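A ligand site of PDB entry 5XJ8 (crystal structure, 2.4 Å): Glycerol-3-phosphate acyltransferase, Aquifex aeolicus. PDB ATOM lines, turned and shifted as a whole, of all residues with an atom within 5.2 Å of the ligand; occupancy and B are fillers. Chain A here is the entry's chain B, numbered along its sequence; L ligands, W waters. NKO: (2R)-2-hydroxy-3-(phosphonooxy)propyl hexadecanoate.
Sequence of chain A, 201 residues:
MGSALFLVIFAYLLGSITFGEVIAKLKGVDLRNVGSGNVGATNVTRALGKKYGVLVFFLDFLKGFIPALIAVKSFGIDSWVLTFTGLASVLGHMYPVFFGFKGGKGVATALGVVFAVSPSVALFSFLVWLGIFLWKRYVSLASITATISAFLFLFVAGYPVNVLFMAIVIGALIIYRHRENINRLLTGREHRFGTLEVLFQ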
ATOM      1  N   SER A  36       5.658  -4.406   6.103  1.00  0.00           N
ATOM      2  CA  SER A  36       6.574  -5.067   7.012  1.00  0.00           C
ATOM      3  C   SER A  36       7.522  -6.036   6.306  1.00  0.00           C
ATOM      4  O   SER A  36       8.487  -6.494   6.927  1.00  0.00           O
ATOM      5  CB  SER A  36       5.803  -5.831   8.087  1.00  0.00           C
ATOM      6  OG  SER A  36       4.928  -6.787   7.508  1.00  0.00           O
ATOM      7  N   ASN A  38       6.593  -8.954   5.592  1.00  0.00           N
ATOM      8  CA  ASN A  38       6.089 -10.261   5.976  1.00  0.00           C
ATOM      9  C   ASN A  38       5.283 -10.889   4.833  1.00  0.00           C
ATOM     10  O   ASN A  38       4.745 -10.182   3.972  1.00  0.00           O
ATOM     11  CB  ASN A  38       5.219 -10.139   7.223  1.00  0.00           C
ATOM     12  CG  ASN A  38       4.818 -11.480   7.793  1.00  0.00           C
ATOM     13  OD1 ASN A  38       5.651 -12.353   8.022  1.00  0.00           O
ATOM     14  ND2 ASN A  38       3.521 -11.655   8.034  1.00  0.00           N
ATOM     15  N   GLY A  40       2.720 -12.844   5.354  1.00  0.00           N
ATOM     16  CA  GLY A  40       1.463 -13.243   5.944  1.00  0.00           C
ATOM     17  C   GLY A  40       0.292 -12.403   5.481  1.00  0.00           C
ATOM     18  O   GLY A  40       0.411 -11.472   4.692  1.00  0.00           O
ATOM     19  N   ALA A  41      -0.882 -12.756   6.028  1.00  0.00           N
ATOM     20  CA  ALA A  41      -2.135 -12.160   5.580  1.00  0.00           C
ATOM     21  C   ALA A  41      -2.171 -10.660   5.798  1.00  0.00           C
ATOM     22  O   ALA A  41      -2.729  -9.918   4.974  1.00  0.00           O
ATOM     23  CB  ALA A  41      -3.313 -12.834   6.295  1.00  0.00           C
ATOM     24  N   THR A  42      -1.584 -10.183   6.896  1.00  0.00           N
ATOM     25  CA  THR A  42      -1.622  -8.757   7.198  1.00  0.00           C
ATOM     26  C   THR A  42      -0.874  -7.950   6.149  1.00  0.00           C
ATOM     27  O   THR A  42      -1.360  -6.901   5.696  1.00  0.00           O
ATOM     28  CB  THR A  42      -1.049  -8.494   8.583  1.00  0.00           C
ATOM     29  OG1 THR A  42      -1.730  -9.294   9.546  1.00  0.00           O
ATOM     30  CG2 THR A  42      -1.204  -7.022   8.953  1.00  0.00           C
ATOM     31  N   ASN A  43       0.299  -8.421   5.733  1.00  0.00           N
ATOM     32  CA  ASN A  43       1.080  -7.690   4.738  1.00  0.00           C
ATOM     33  C   ASN A  43       0.570  -7.952   3.324  1.00  0.00           C
ATOM     34  O   ASN A  43       0.745  -7.093   2.447  1.00  0.00           O
ATOM     35  CB  ASN A  43       2.559  -8.050   4.841  1.00  0.00           C
ATOM     36  CG  ASN A  43       3.466  -6.945   4.345  1.00  0.00           C
ATOM     37  OD1 ASN A  43       3.271  -5.773   4.664  1.00  0.00           O
ATOM     38  ND2 ASN A  43       4.459  -7.316   3.542  1.00  0.00           N
ATOM     39  N   ARG A  46      -1.868  -5.222   2.694  1.00  0.00           N
ATOM     40  CA  ARG A  46      -1.253  -3.965   2.277  1.00  0.00           C
ATOM     41  C   ARG A  46      -0.847  -4.013   0.816  1.00  0.00           C
ATOM     42  O   ARG A  46      -1.032  -3.037   0.072  1.00  0.00           O
ATOM     43  CB  ARG A  46      -0.038  -3.653   3.149  1.00  0.00           C
ATOM     44  CG  ARG A  46      -0.285  -3.682   4.647  1.00  0.00           C
ATOM     45  CD  ARG A  46       0.977  -3.284   5.392  1.00  0.00           C
ATOM     46  NE  ARG A  46       0.782  -3.248   6.844  1.00  0.00           N
ATOM     47  CZ  ARG A  46       1.177  -4.209   7.683  1.00  0.00           C
ATOM     48  NH1 ARG A  46       0.952  -4.088   8.981  1.00  0.00           N
ATOM     49  NH2 ARG A  46       1.783  -5.293   7.210  1.00  0.00           N
ATOM     50  N   PHE A  57      -5.293 -15.555   4.604  1.00  0.00           N
ATOM     51  CA  PHE A  57      -5.589 -15.941   5.976  1.00  0.00           C
ATOM     52  C   PHE A  57      -6.276 -17.305   6.033  1.00  0.00           C
ATOM     53  O   PHE A  57      -5.969 -18.124   6.894  1.00  0.00           O
ATOM     54  CB  PHE A  57      -6.475 -14.882   6.648  1.00  0.00           C
ATOM     55  CG  PHE A  57      -7.179 -15.383   7.880  1.00  0.00           C
ATOM     56  CD1 PHE A  57      -6.533 -15.456   9.094  1.00  0.00           C
ATOM     57  CD2 PHE A  57      -8.512 -15.785   7.821  1.00  0.00           C
ATOM     58  CE1 PHE A  57      -7.177 -15.915  10.237  1.00  0.00           C
ATOM     59  CE2 PHE A  57      -9.170 -16.247   8.948  1.00  0.00           C
ATOM     60  CZ  PHE A  57      -8.497 -16.311  10.151  1.00  0.00           C
ATOM     61  N   LYS A 105       5.034 -15.205  10.550  1.00  0.00           N
ATOM     62  CA  LYS A 105       5.035 -15.239  12.005  1.00  0.00           C
ATOM     63  C   LYS A 105       4.032 -16.233  12.576  1.00  0.00           C
ATOM     64  O   LYS A 105       3.937 -16.362  13.798  1.00  0.00           O
ATOM     65  CB  LYS A 105       4.784 -13.820  12.539  1.00  0.00           C
ATOM     66  CG  LYS A 105       5.358 -12.766  11.604  1.00  0.00           C
ATOM     67  CD  LYS A 105       5.600 -11.412  12.269  1.00  0.00           C
ATOM     68  CE  LYS A 105       6.500 -10.555  11.398  1.00  0.00           C
ATOM     69  NZ  LYS A 105       6.240  -9.092  11.538  1.00  0.00           N
ATOM     70  N   VAL A 107       0.656 -16.677  12.797  1.00  0.00           N
ATOM     71  CA  VAL A 107      -0.547 -16.395  13.589  1.00  0.00           C
ATOM     72  C   VAL A 107      -1.772 -17.068  12.990  1.00  0.00           C
ATOM     73  O   VAL A 107      -2.598 -17.636  13.720  1.00  0.00           O
ATOM     74  CB  VAL A 107      -0.743 -14.873  13.727  1.00  0.00           C
ATOM     75  CG1 VAL A 107      -2.033 -14.581  14.486  1.00  0.00           C
ATOM     76  CG2 VAL A 107       0.459 -14.254  14.438  1.00  0.00           C
ATOM     77  N   ALA A 108      -1.917 -17.032  11.662  1.00  0.00           N
ATOM     78  CA  ALA A 108      -3.074 -17.659  11.035  1.00  0.00           C
ATOM     79  C   ALA A 108      -3.010 -19.175  11.134  1.00  0.00           C
ATOM     80  O   ALA A 108      -4.022 -19.835  11.414  1.00  0.00           O
ATOM     81  CB  ALA A 108      -3.173 -17.230   9.571  1.00  0.00           C
ATOM     82  N   ALA A 110      -1.418 -20.935  13.421  1.00  0.00           N
ATOM     83  CA  ALA A 110      -1.627 -21.316  14.810  1.00  0.00           C
ATOM     84  C   ALA A 110      -3.099 -21.275  15.174  1.00  0.00           C
ATOM     85  O   ALA A 110      -3.582 -22.121  15.929  1.00  0.00           O
ATOM     86  CB  ALA A 110      -0.820 -20.411  15.744  1.00  0.00           C
ATOM     87  N   LEU A 111      -3.837 -20.288  14.647  1.00  0.00           N
ATOM     88  CA  LEU A 111      -5.274 -20.254  14.873  1.00  0.00           C
ATOM     89  C   LEU A 111      -5.967 -21.444  14.236  1.00  0.00           C
ATOM     90  O   LEU A 111      -6.983 -21.930  14.752  1.00  0.00           O
ATOM     91  CB  LEU A 111      -5.857 -18.947  14.344  1.00  0.00           C
ATOM     92  CG  LEU A 111      -7.311 -18.656  14.734  1.00  0.00           C
ATOM     93  CD1 LEU A 111      -7.435 -18.413  16.228  1.00  0.00           C
ATOM     94  CD2 LEU A 111      -7.862 -17.482  13.949  1.00  0.00           C
ATOM     95  N   VAL A 114      -5.432 -24.270  16.765  1.00  0.00           N
ATOM     96  CA  VAL A 114      -6.308 -24.112  17.915  1.00  0.00           C
ATOM     97  C   VAL A 114      -7.753 -24.450  17.536  1.00  0.00           C
ATOM     98  O   VAL A 114      -8.482 -25.065  18.325  1.00  0.00           O
ATOM     99  CB  VAL A 114      -6.207 -22.676  18.470  1.00  0.00           C
ATOM    100  CG1 VAL A 114      -7.180 -22.467  19.616  1.00  0.00           C
ATOM    101  CG2 VAL A 114      -4.784 -22.405  18.937  1.00  0.00           C
ATOM    102  N   SER A 125     -10.331 -16.233  20.939  1.00  0.00           N
ATOM    103  CA  SER A 125      -9.052 -15.610  20.634  1.00  0.00           C
ATOM    104  C   SER A 125      -9.158 -14.697  19.427  1.00  0.00           C
ATOM    105  O   SER A 125      -8.535 -13.632  19.381  1.00  0.00           O
ATOM    106  CB  SER A 125      -7.982 -16.676  20.423  1.00  0.00           C
ATOM    107  OG  SER A 125      -7.968 -17.601  21.499  1.00  0.00           O
ATOM    108  N   PHE A 126      -9.941 -15.104  18.421  1.00  0.00           N
ATOM    109  CA  PHE A 126     -10.168 -14.228  17.274  1.00  0.00           C
ATOM    110  C   PHE A 126     -10.986 -13.005  17.662  1.00  0.00           C
ATOM    111  O   PHE A 126     -10.759 -11.911  17.136  1.00  0.00           O
ATOM    112  CB  PHE A 126     -10.863 -14.999  16.144  1.00  0.00           C
ATOM    113  CG  PHE A 126     -11.038 -14.188  14.898  1.00  0.00           C
ATOM    114  CD1 PHE A 126      -9.972 -14.001  14.034  1.00  0.00           C
ATOM    115  CD2 PHE A 126     -12.241 -13.595  14.595  1.00  0.00           C
ATOM    116  CE1 PHE A 126     -10.116 -13.246  12.880  1.00  0.00           C
ATOM    117  CE2 PHE A 126     -12.401 -12.846  13.443  1.00  0.00           C
ATOM    118  CZ  PHE A 126     -11.331 -12.666  12.591  1.00  0.00           C
ATOM    119  N   TRP A 129      -8.526 -10.863  19.319  1.00  0.00           N
ATOM    120  CA  TRP A 129      -7.712 -10.230  18.287  1.00  0.00           C
ATOM    121  C   TRP A 129      -8.458  -9.092  17.614  1.00  0.00           C
ATOM    122  O   TRP A 129      -7.874  -8.035  17.334  1.00  0.00           O
ATOM    123  CB  TRP A 129      -7.279 -11.267  17.254  1.00  0.00           C
ATOM    124  CG  TRP A 129      -6.428 -10.713  16.153  1.00  0.00           C
ATOM    125  CD1 TRP A 129      -5.070 -10.633  16.135  1.00  0.00           C
ATOM    126  CD2 TRP A 129      -6.875 -10.148  14.915  1.00  0.00           C
ATOM    127  NE1 TRP A 129      -4.642 -10.055  14.957  1.00  0.00           N
ATOM    128  CE2 TRP A 129      -5.731  -9.753  14.196  1.00  0.00           C
ATOM    129  CE3 TRP A 129      -8.134  -9.947  14.338  1.00  0.00           C
ATOM    130  CZ2 TRP A 129      -5.809  -9.163  12.936  1.00  0.00           C
ATOM    131  CZ3 TRP A 129      -8.215  -9.359  13.096  1.00  0.00           C
ATOM    132  CH2 TRP A 129      -7.064  -8.978  12.400  1.00  0.00           C
ATOM    133  N   VAL A 139      -2.129  -4.564  14.063  1.00  0.00           N
ATOM    134  CA  VAL A 139      -2.378  -6.001  13.936  1.00  0.00           C
ATOM    135  C   VAL A 139      -1.419  -6.787  14.807  1.00  0.00           C
ATOM    136  O   VAL A 139      -1.800  -7.783  15.436  1.00  0.00           O
ATOM    137  CB  VAL A 139      -2.277  -6.424  12.460  1.00  0.00           C
ATOM    138  CG1 VAL A 139      -2.377  -7.939  12.339  1.00  0.00           C
ATOM    139  CG2 VAL A 139      -3.368  -5.760  11.637  1.00  0.00           C
ATOM    140  N   SER A 140      -0.162  -6.352  14.886  1.00  0.00           N
ATOM    141  CA  SER A 140       0.840  -7.079  15.665  1.00  0.00           C
ATOM    142  C   SER A 140       0.491  -7.088  17.140  1.00  0.00           C
ATOM    143  O   SER A 140       0.676  -8.105  17.826  1.00  0.00           O
ATOM    144  CB  SER A 140       2.224  -6.482  15.447  1.00  0.00           C
ATOM    145  OG  SER A 140       2.299  -5.172  15.985  1.00  0.00           O
ATOM    146  N   SER A 143      -2.349  -9.527  17.535  1.00  0.00           N
ATOM    147  CA  SER A 143      -1.887 -10.909  17.402  1.00  0.00           C
ATOM    148  C   SER A 143      -1.137 -11.368  18.646  1.00  0.00           C
ATOM    149  O   SER A 143      -1.334 -12.500  19.113  1.00  0.00           O
ATOM    150  CB  SER A 143      -1.009 -11.052  16.165  1.00  0.00           C
ATOM    151  OG  SER A 143      -1.771 -10.953  14.979  1.00  0.00           O
ATOM    152  N   ALA A 146      -3.867 -11.733  21.444  1.00  0.00           N
ATOM    153  CA  ALA A 146      -4.713 -12.894  21.220  1.00  0.00           C
ATOM    154  C   ALA A 146      -3.930 -14.188  21.380  1.00  0.00           C
ATOM    155  O   ALA A 146      -4.497 -15.212  21.786  1.00  0.00           O
ATOM    156  CB  ALA A 146      -5.355 -12.828  19.827  1.00  0.00           C
ATOM    157  N   THR A 147      -2.637 -14.179  21.055  1.00  0.00           N
ATOM    158  CA  THR A 147      -1.823 -15.369  21.259  1.00  0.00           C
ATOM    159  C   THR A 147      -1.705 -15.703  22.741  1.00  0.00           C
ATOM    160  O   THR A 147      -1.795 -16.869  23.134  1.00  0.00           O
ATOM    161  CB  THR A 147      -0.430 -15.162  20.643  1.00  0.00           C
ATOM    162  OG1 THR A 147      -0.570 -14.938  19.231  1.00  0.00           O
ATOM    163  CG2 THR A 147       0.433 -16.382  20.864  1.00  0.00           C
ATOM    164  N   ALA A 150      -5.109 -16.870  23.950  1.00  0.00           N
ATOM    165  CA  ALA A 150      -5.405 -18.221  23.495  1.00  0.00           C
ATOM    166  C   ALA A 150      -4.827 -19.265  24.447  1.00  0.00           C
ATOM    167  O   ALA A 150      -5.460 -20.285  24.722  1.00  0.00           O
ATOM    168  CB  ALA A 150      -4.875 -18.434  22.082  1.00  0.00           C
ATOM    169  N   ALA A 167       0.825 -24.986  23.015  1.00  0.00           N
ATOM    170  CA  ALA A 167       0.435 -23.579  22.957  1.00  0.00           C
ATOM    171  C   ALA A 167       1.554 -22.670  23.451  1.00  0.00           C
ATOM    172  O   ALA A 167       1.754 -21.576  22.908  1.00  0.00           O
ATOM    173  CB  ALA A 167      -0.833 -23.366  23.780  1.00  0.00           C
ATOM    174  N   ILE A 170       4.333 -22.633  20.652  1.00  0.00           N
ATOM    175  CA  ILE A 170       3.814 -21.875  19.505  1.00  0.00           C
ATOM    176  C   ILE A 170       3.698 -20.397  19.865  1.00  0.00           C
ATOM    177  O   ILE A 170       4.116 -19.527  19.095  1.00  0.00           O
ATOM    178  CB  ILE A 170       2.465 -22.452  19.050  1.00  0.00           C
ATOM    179  CG1 ILE A 170       2.669 -23.773  18.308  1.00  0.00           C
ATOM    180  CG2 ILE A 170       1.726 -21.451  18.169  1.00  0.00           C
ATOM    181  CD1 ILE A 170       1.372 -24.467  17.953  1.00  0.00           C
ATOM    182  N   GLY A 171       3.143 -20.106  21.042  1.00  0.00           N
ATOM    183  CA  GLY A 171       3.005 -18.722  21.455  1.00  0.00           C
ATOM    184  C   GLY A 171       4.341 -18.025  21.652  1.00  0.00           C
ATOM    185  O   GLY A 171       4.520 -16.873  21.238  1.00  0.00           O
ATOM    186  N   ILE A 174       5.615 -17.239  18.272  1.00  0.00           N
ATOM    187  CA  ILE A 174       4.906 -16.150  17.617  1.00  0.00           C
ATOM    188  C   ILE A 174       5.402 -14.806  18.139  1.00  0.00           C
ATOM    189  O   ILE A 174       5.679 -13.884  17.361  1.00  0.00           O
ATOM    190  CB  ILE A 174       3.386 -16.298  17.820  1.00  0.00           C
ATOM    191  CG1 ILE A 174       2.844 -17.452  16.973  1.00  0.00           C
ATOM    192  CG2 ILE A 174       2.670 -14.998  17.478  1.00  0.00           C
ATOM    193  CD1 ILE A 174       1.388 -17.770  17.222  1.00  0.00           C
ATOM    194  N   HIS A 178       7.656 -11.683  16.308  1.00  0.00           N
ATOM    195  CA  HIS A 178       7.123 -10.336  16.321  1.00  0.00           C
ATOM    196  C   HIS A 178       8.095  -9.338  16.955  1.00  0.00           C
ATOM    197  O   HIS A 178       7.711  -8.184  17.188  1.00  0.00           O
ATOM    198  CB  HIS A 178       5.785 -10.289  17.066  1.00  0.00           C
ATOM    199  CG  HIS A 178       4.609 -10.720  16.238  1.00  0.00           C
ATOM    200  ND1 HIS A 178       4.233 -12.034  16.117  1.00  0.00           N
ATOM    201  CD2 HIS A 178       3.748 -10.000  15.484  1.00  0.00           C
ATOM    202  CE1 HIS A 178       3.170 -12.110  15.331  1.00  0.00           C
ATOM    203  NE2 HIS A 178       2.855 -10.890  14.934  1.00  0.00           N
ATOM    204  N   ASN A 181       8.232  -6.221  15.122  1.00  0.00           N
ATOM    205  CA  ASN A 181       7.041  -5.430  15.377  1.00  0.00           C
ATOM    206  C   ASN A 181       7.078  -4.813  16.771  1.00  0.00           C
ATOM    207  O   ASN A 181       6.661  -3.667  16.968  1.00  0.00           O
ATOM    208  CB  ASN A 181       5.790  -6.280  15.204  1.00  0.00           C
ATOM    209  CG  ASN A 181       5.765  -7.018  13.879  1.00  0.00           C
ATOM    210  OD1 ASN A 181       6.338  -8.111  13.749  1.00  0.00           O
ATOM    211  ND2 ASN A 181       5.099  -6.440  12.887  1.00  0.00           N
ATOM    212  N   ARG A 184       9.278  -1.889  16.734  1.00  0.00           N
ATOM    213  CA  ARG A 184       8.654  -0.770  16.052  1.00  0.00           C
ATOM    214  C   ARG A 184       7.545  -0.148  16.892  1.00  0.00           C
ATOM    215  O   ARG A 184       7.336   1.070  16.848  1.00  0.00           O
ATOM    216  CB  ARG A 184       8.108  -1.213  14.694  1.00  0.00           C
ATOM    217  CG  ARG A 184       9.175  -1.381  13.619  1.00  0.00           C
ATOM    218  CD  ARG A 184       8.561  -1.412  12.236  1.00  0.00           C
ATOM    219  NE  ARG A 184       7.751  -2.607  12.014  1.00  0.00           N
ATOM    220  CZ  ARG A 184       8.237  -3.771  11.585  1.00  0.00           C
ATOM    221  NH1 ARG A 184       9.530  -3.886  11.314  1.00  0.00           N
ATOM    222  NH2 ARG A 184       7.432  -4.812  11.422  1.00  0.00           N
ATOM    223  N   GLU A 190       5.792   1.318  14.065  1.00  0.00           N
ATOM    224  CA  GLU A 190       5.031   0.193  13.543  1.00  0.00           C
ATOM    225  C   GLU A 190       3.970   0.656  12.560  1.00  0.00           C
ATOM    226  O   GLU A 190       3.337   1.695  12.754  1.00  0.00           O
ATOM    227  CB  GLU A 190       4.396  -0.599  14.693  1.00  0.00           C
ATOM    228  CG  GLU A 190       3.389  -1.655  14.252  1.00  0.00           C
ATOM    229  CD  GLU A 190       4.033  -2.924  13.731  1.00  0.00           C
ATOM    230  OE1 GLU A 190       3.559  -4.019  14.097  1.00  0.00           O
ATOM    231  OE2 GLU A 190       4.997  -2.843  12.939  1.00  0.00           O
HETATM  232  OAA NKO L   1       2.586  -5.982  10.325  1.00  0.00           O
HETATM  233  OAB NKO L   1       2.778  -7.704   8.485  1.00  0.00           O
HETATM  234  PAC NKO L   1       2.815  -7.425   9.991  1.00  0.00           P
HETATM  235  OAD NKO L   1       4.143  -7.952  10.534  1.00  0.00           O
HETATM  236  OAE NKO L   1      -0.443 -11.605   9.187  1.00  0.00           O
HETATM  237  OAF NKO L   1       1.681  -8.326  10.646  1.00  0.00           O
HETATM  238  CAG NKO L   1       1.609  -8.758  12.018  1.00  0.00           C
HETATM  239  CAH NKO L   1       0.717  -9.975  12.105  1.00  0.00           C
HETATM  240  CAI NKO L   1       1.197 -11.106  11.240  1.00  0.00           C
HETATM  241  OAJ NKO L   1       0.130 -12.087  11.297  1.00  0.00           O
HETATM  242  CAK NKO L   1      -0.631 -12.211  10.199  1.00  0.00           C
HETATM  243  CAL NKO L   1      -1.734 -13.208  10.413  1.00  0.00           C
HETATM  244  CAM NKO L   1      -3.043 -12.548  10.800  1.00  0.00           C
HETATM  245  CAN NKO L   1      -4.208 -13.522  10.833  1.00  0.00           C
HETATM  246  CAO NKO L   1      -5.503 -12.905  11.353  1.00  0.00           C
HETATM  247  CAP NKO L   1      -5.616 -12.855  12.864  1.00  0.00           C
HETATM  248  CAQ NKO L   1      -6.056 -14.168  13.490  1.00  0.00           C
HETATM  249  CAR NKO L   1      -6.478 -14.058  14.951  1.00  0.00           C
HETATM  250  CAS NKO L   1      -5.351 -14.158  15.961  1.00  0.00           C
HETATM  251  CAT NKO L   1      -5.321 -15.464  16.737  1.00  0.00           C
HETATM  252  CAU NKO L   1      -4.119 -15.622  17.653  1.00  0.00           C
HETATM  253  CAV NKO L   1      -3.207 -16.778  17.275  1.00  0.00           C
HETATM  254  CAW NKO L   1      -3.479 -18.097  17.997  1.00  0.00           C
HETATM  255  CAX NKO L   1      -2.464 -18.404  19.082  1.00  0.00           C
HETATM  256  CAY NKO L   1      -2.355 -19.888  19.420  1.00  0.00           C
HETATM  257  CAZ NKO L   1      -1.277 -20.191  20.434  1.00  0.00           C
HETATM  258  OBA NKO L   1       0.646 -10.413  13.465  1.00  0.00           O
HETATM  259  O   HOH W   1       1.586  -5.030  12.609  1.00  0.00           O
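Water W1 lies within hydrogen-bond range of an oxygen (OAA) of the ligand (2.7 Å), the side-chain carboxylate (OE1) of Glu 190 (2.7 Å) and the backbone NH (N) of Ser 140 (3.2 Å).
The side-chain hydroxyl (OG) of Ser 36 sits at hydrogen-bond distance from an oxygen (OAB) of the ligand, at 2.5 Å. NZ of Lys 105 is in salt-bridge range of OAD of the ligand (2.6 Å). An oxygen (OAE) of the ligand is in hydrogen-bond range of the backbone NH (N) of Thr 42 (2.9 Å). OG1 of Thr 42 lies within hydrogen-bond range of OAE of the ligand (2.7 Å). An oxygen (OBA) of the ligand is in hydrogen-bond range of a ring nitrogen (NE2) of His 178. The guanidinium group of Arg 46 lies within salt-bridge range of an oxygen (OAA) of the ligand (2.8 Å). OBA of the ligand lies within hydrogen-bond range of OG of Ser 143, 2.9 Å away. The side-chain amide nitrogen (ND2) of Asn 181 lies within hydrogen-bond range of an oxygen (OAD) of the ligand (3.0 Å). N of Ala 41 is in hydrogen-bond range of OAE of the ligand (3.4 Å).
The side-chain hydroxyl (OG) of Ser 36 is in hydrogen-bond range of the guanidinium group (NH2) of Arg 46, at 3.5 Å. The backbone NH (N) of Ser 36 lies within hydrogen-bond range of the side-chain amide oxygen (OD1) of Asn 43 (3.1 Å). The side-chain amino group of Lys 105 sits at hydrogen-bond distance from the side-chain amide oxygen of Asn 181 (2.4 Å). The side-chain hydroxyl (OG) of Ser 143 is in hydrogen-bond range of the indole nitrogen (NE1) of Trp 129. The backbone carbonyl oxygen of Ser 143 sits at hydrogen-bond distance from the side-chain hydroxyl of Thr 147 (2.6 Å). ND2 of Asn 181 lies within hydrogen-bond range of OE1 of Glu 190, 3.1 Å away. ND2 of Asn 181 lies close to NH2 of Arg 184 (3.2 Å). ND2 of Asn 38 lies close to N of Gly 40, 3.0 Å away.
Merely in contact with the ligand: Asn 38 (3.7 Å), Gly 40 (3.9 Å), Asn 43 (3.7 Å), Phe 57 (3.5 Å), Val 107 (3.7 Å), Leu 111 (3.7 Å), Val 114 (3.5 Å), Phe 126 (3.6 Å), Trp 129 (3.4 Å), Val 139 (3.7 Å), Ser 140 (3.999 Å), Ala 146 (3.7 Å), Thr 147 (3.8 Å), Ala 150 (3.8 Å) and Ile 170 (3.97 Å). Hydrophobic or aromatic side chains within 4 Å of the ligand: Phe 57, Val 107, Leu 111, Val 114, Phe 126, Trp 129, Val 139, Ala 146, Ala 150, Ile 170 and His 178. 23 residues have an atom within 4 Å of the ligand: Ser 36, Asn 38, Gly 40, Ala 41, Thr 42, Asn 43, Arg 46, Phe 57, Lys 105, Val 107, Leu 111, Val 114, Phe 126, Trp 129, Val 139, Ser 140, Ser 143, Ala 146, Thr 147, Ala 150, Ile 170, His 178 and Asn 181. The nearest printed residue that does not touch the ligand is Ala 110 (4.02 Å).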
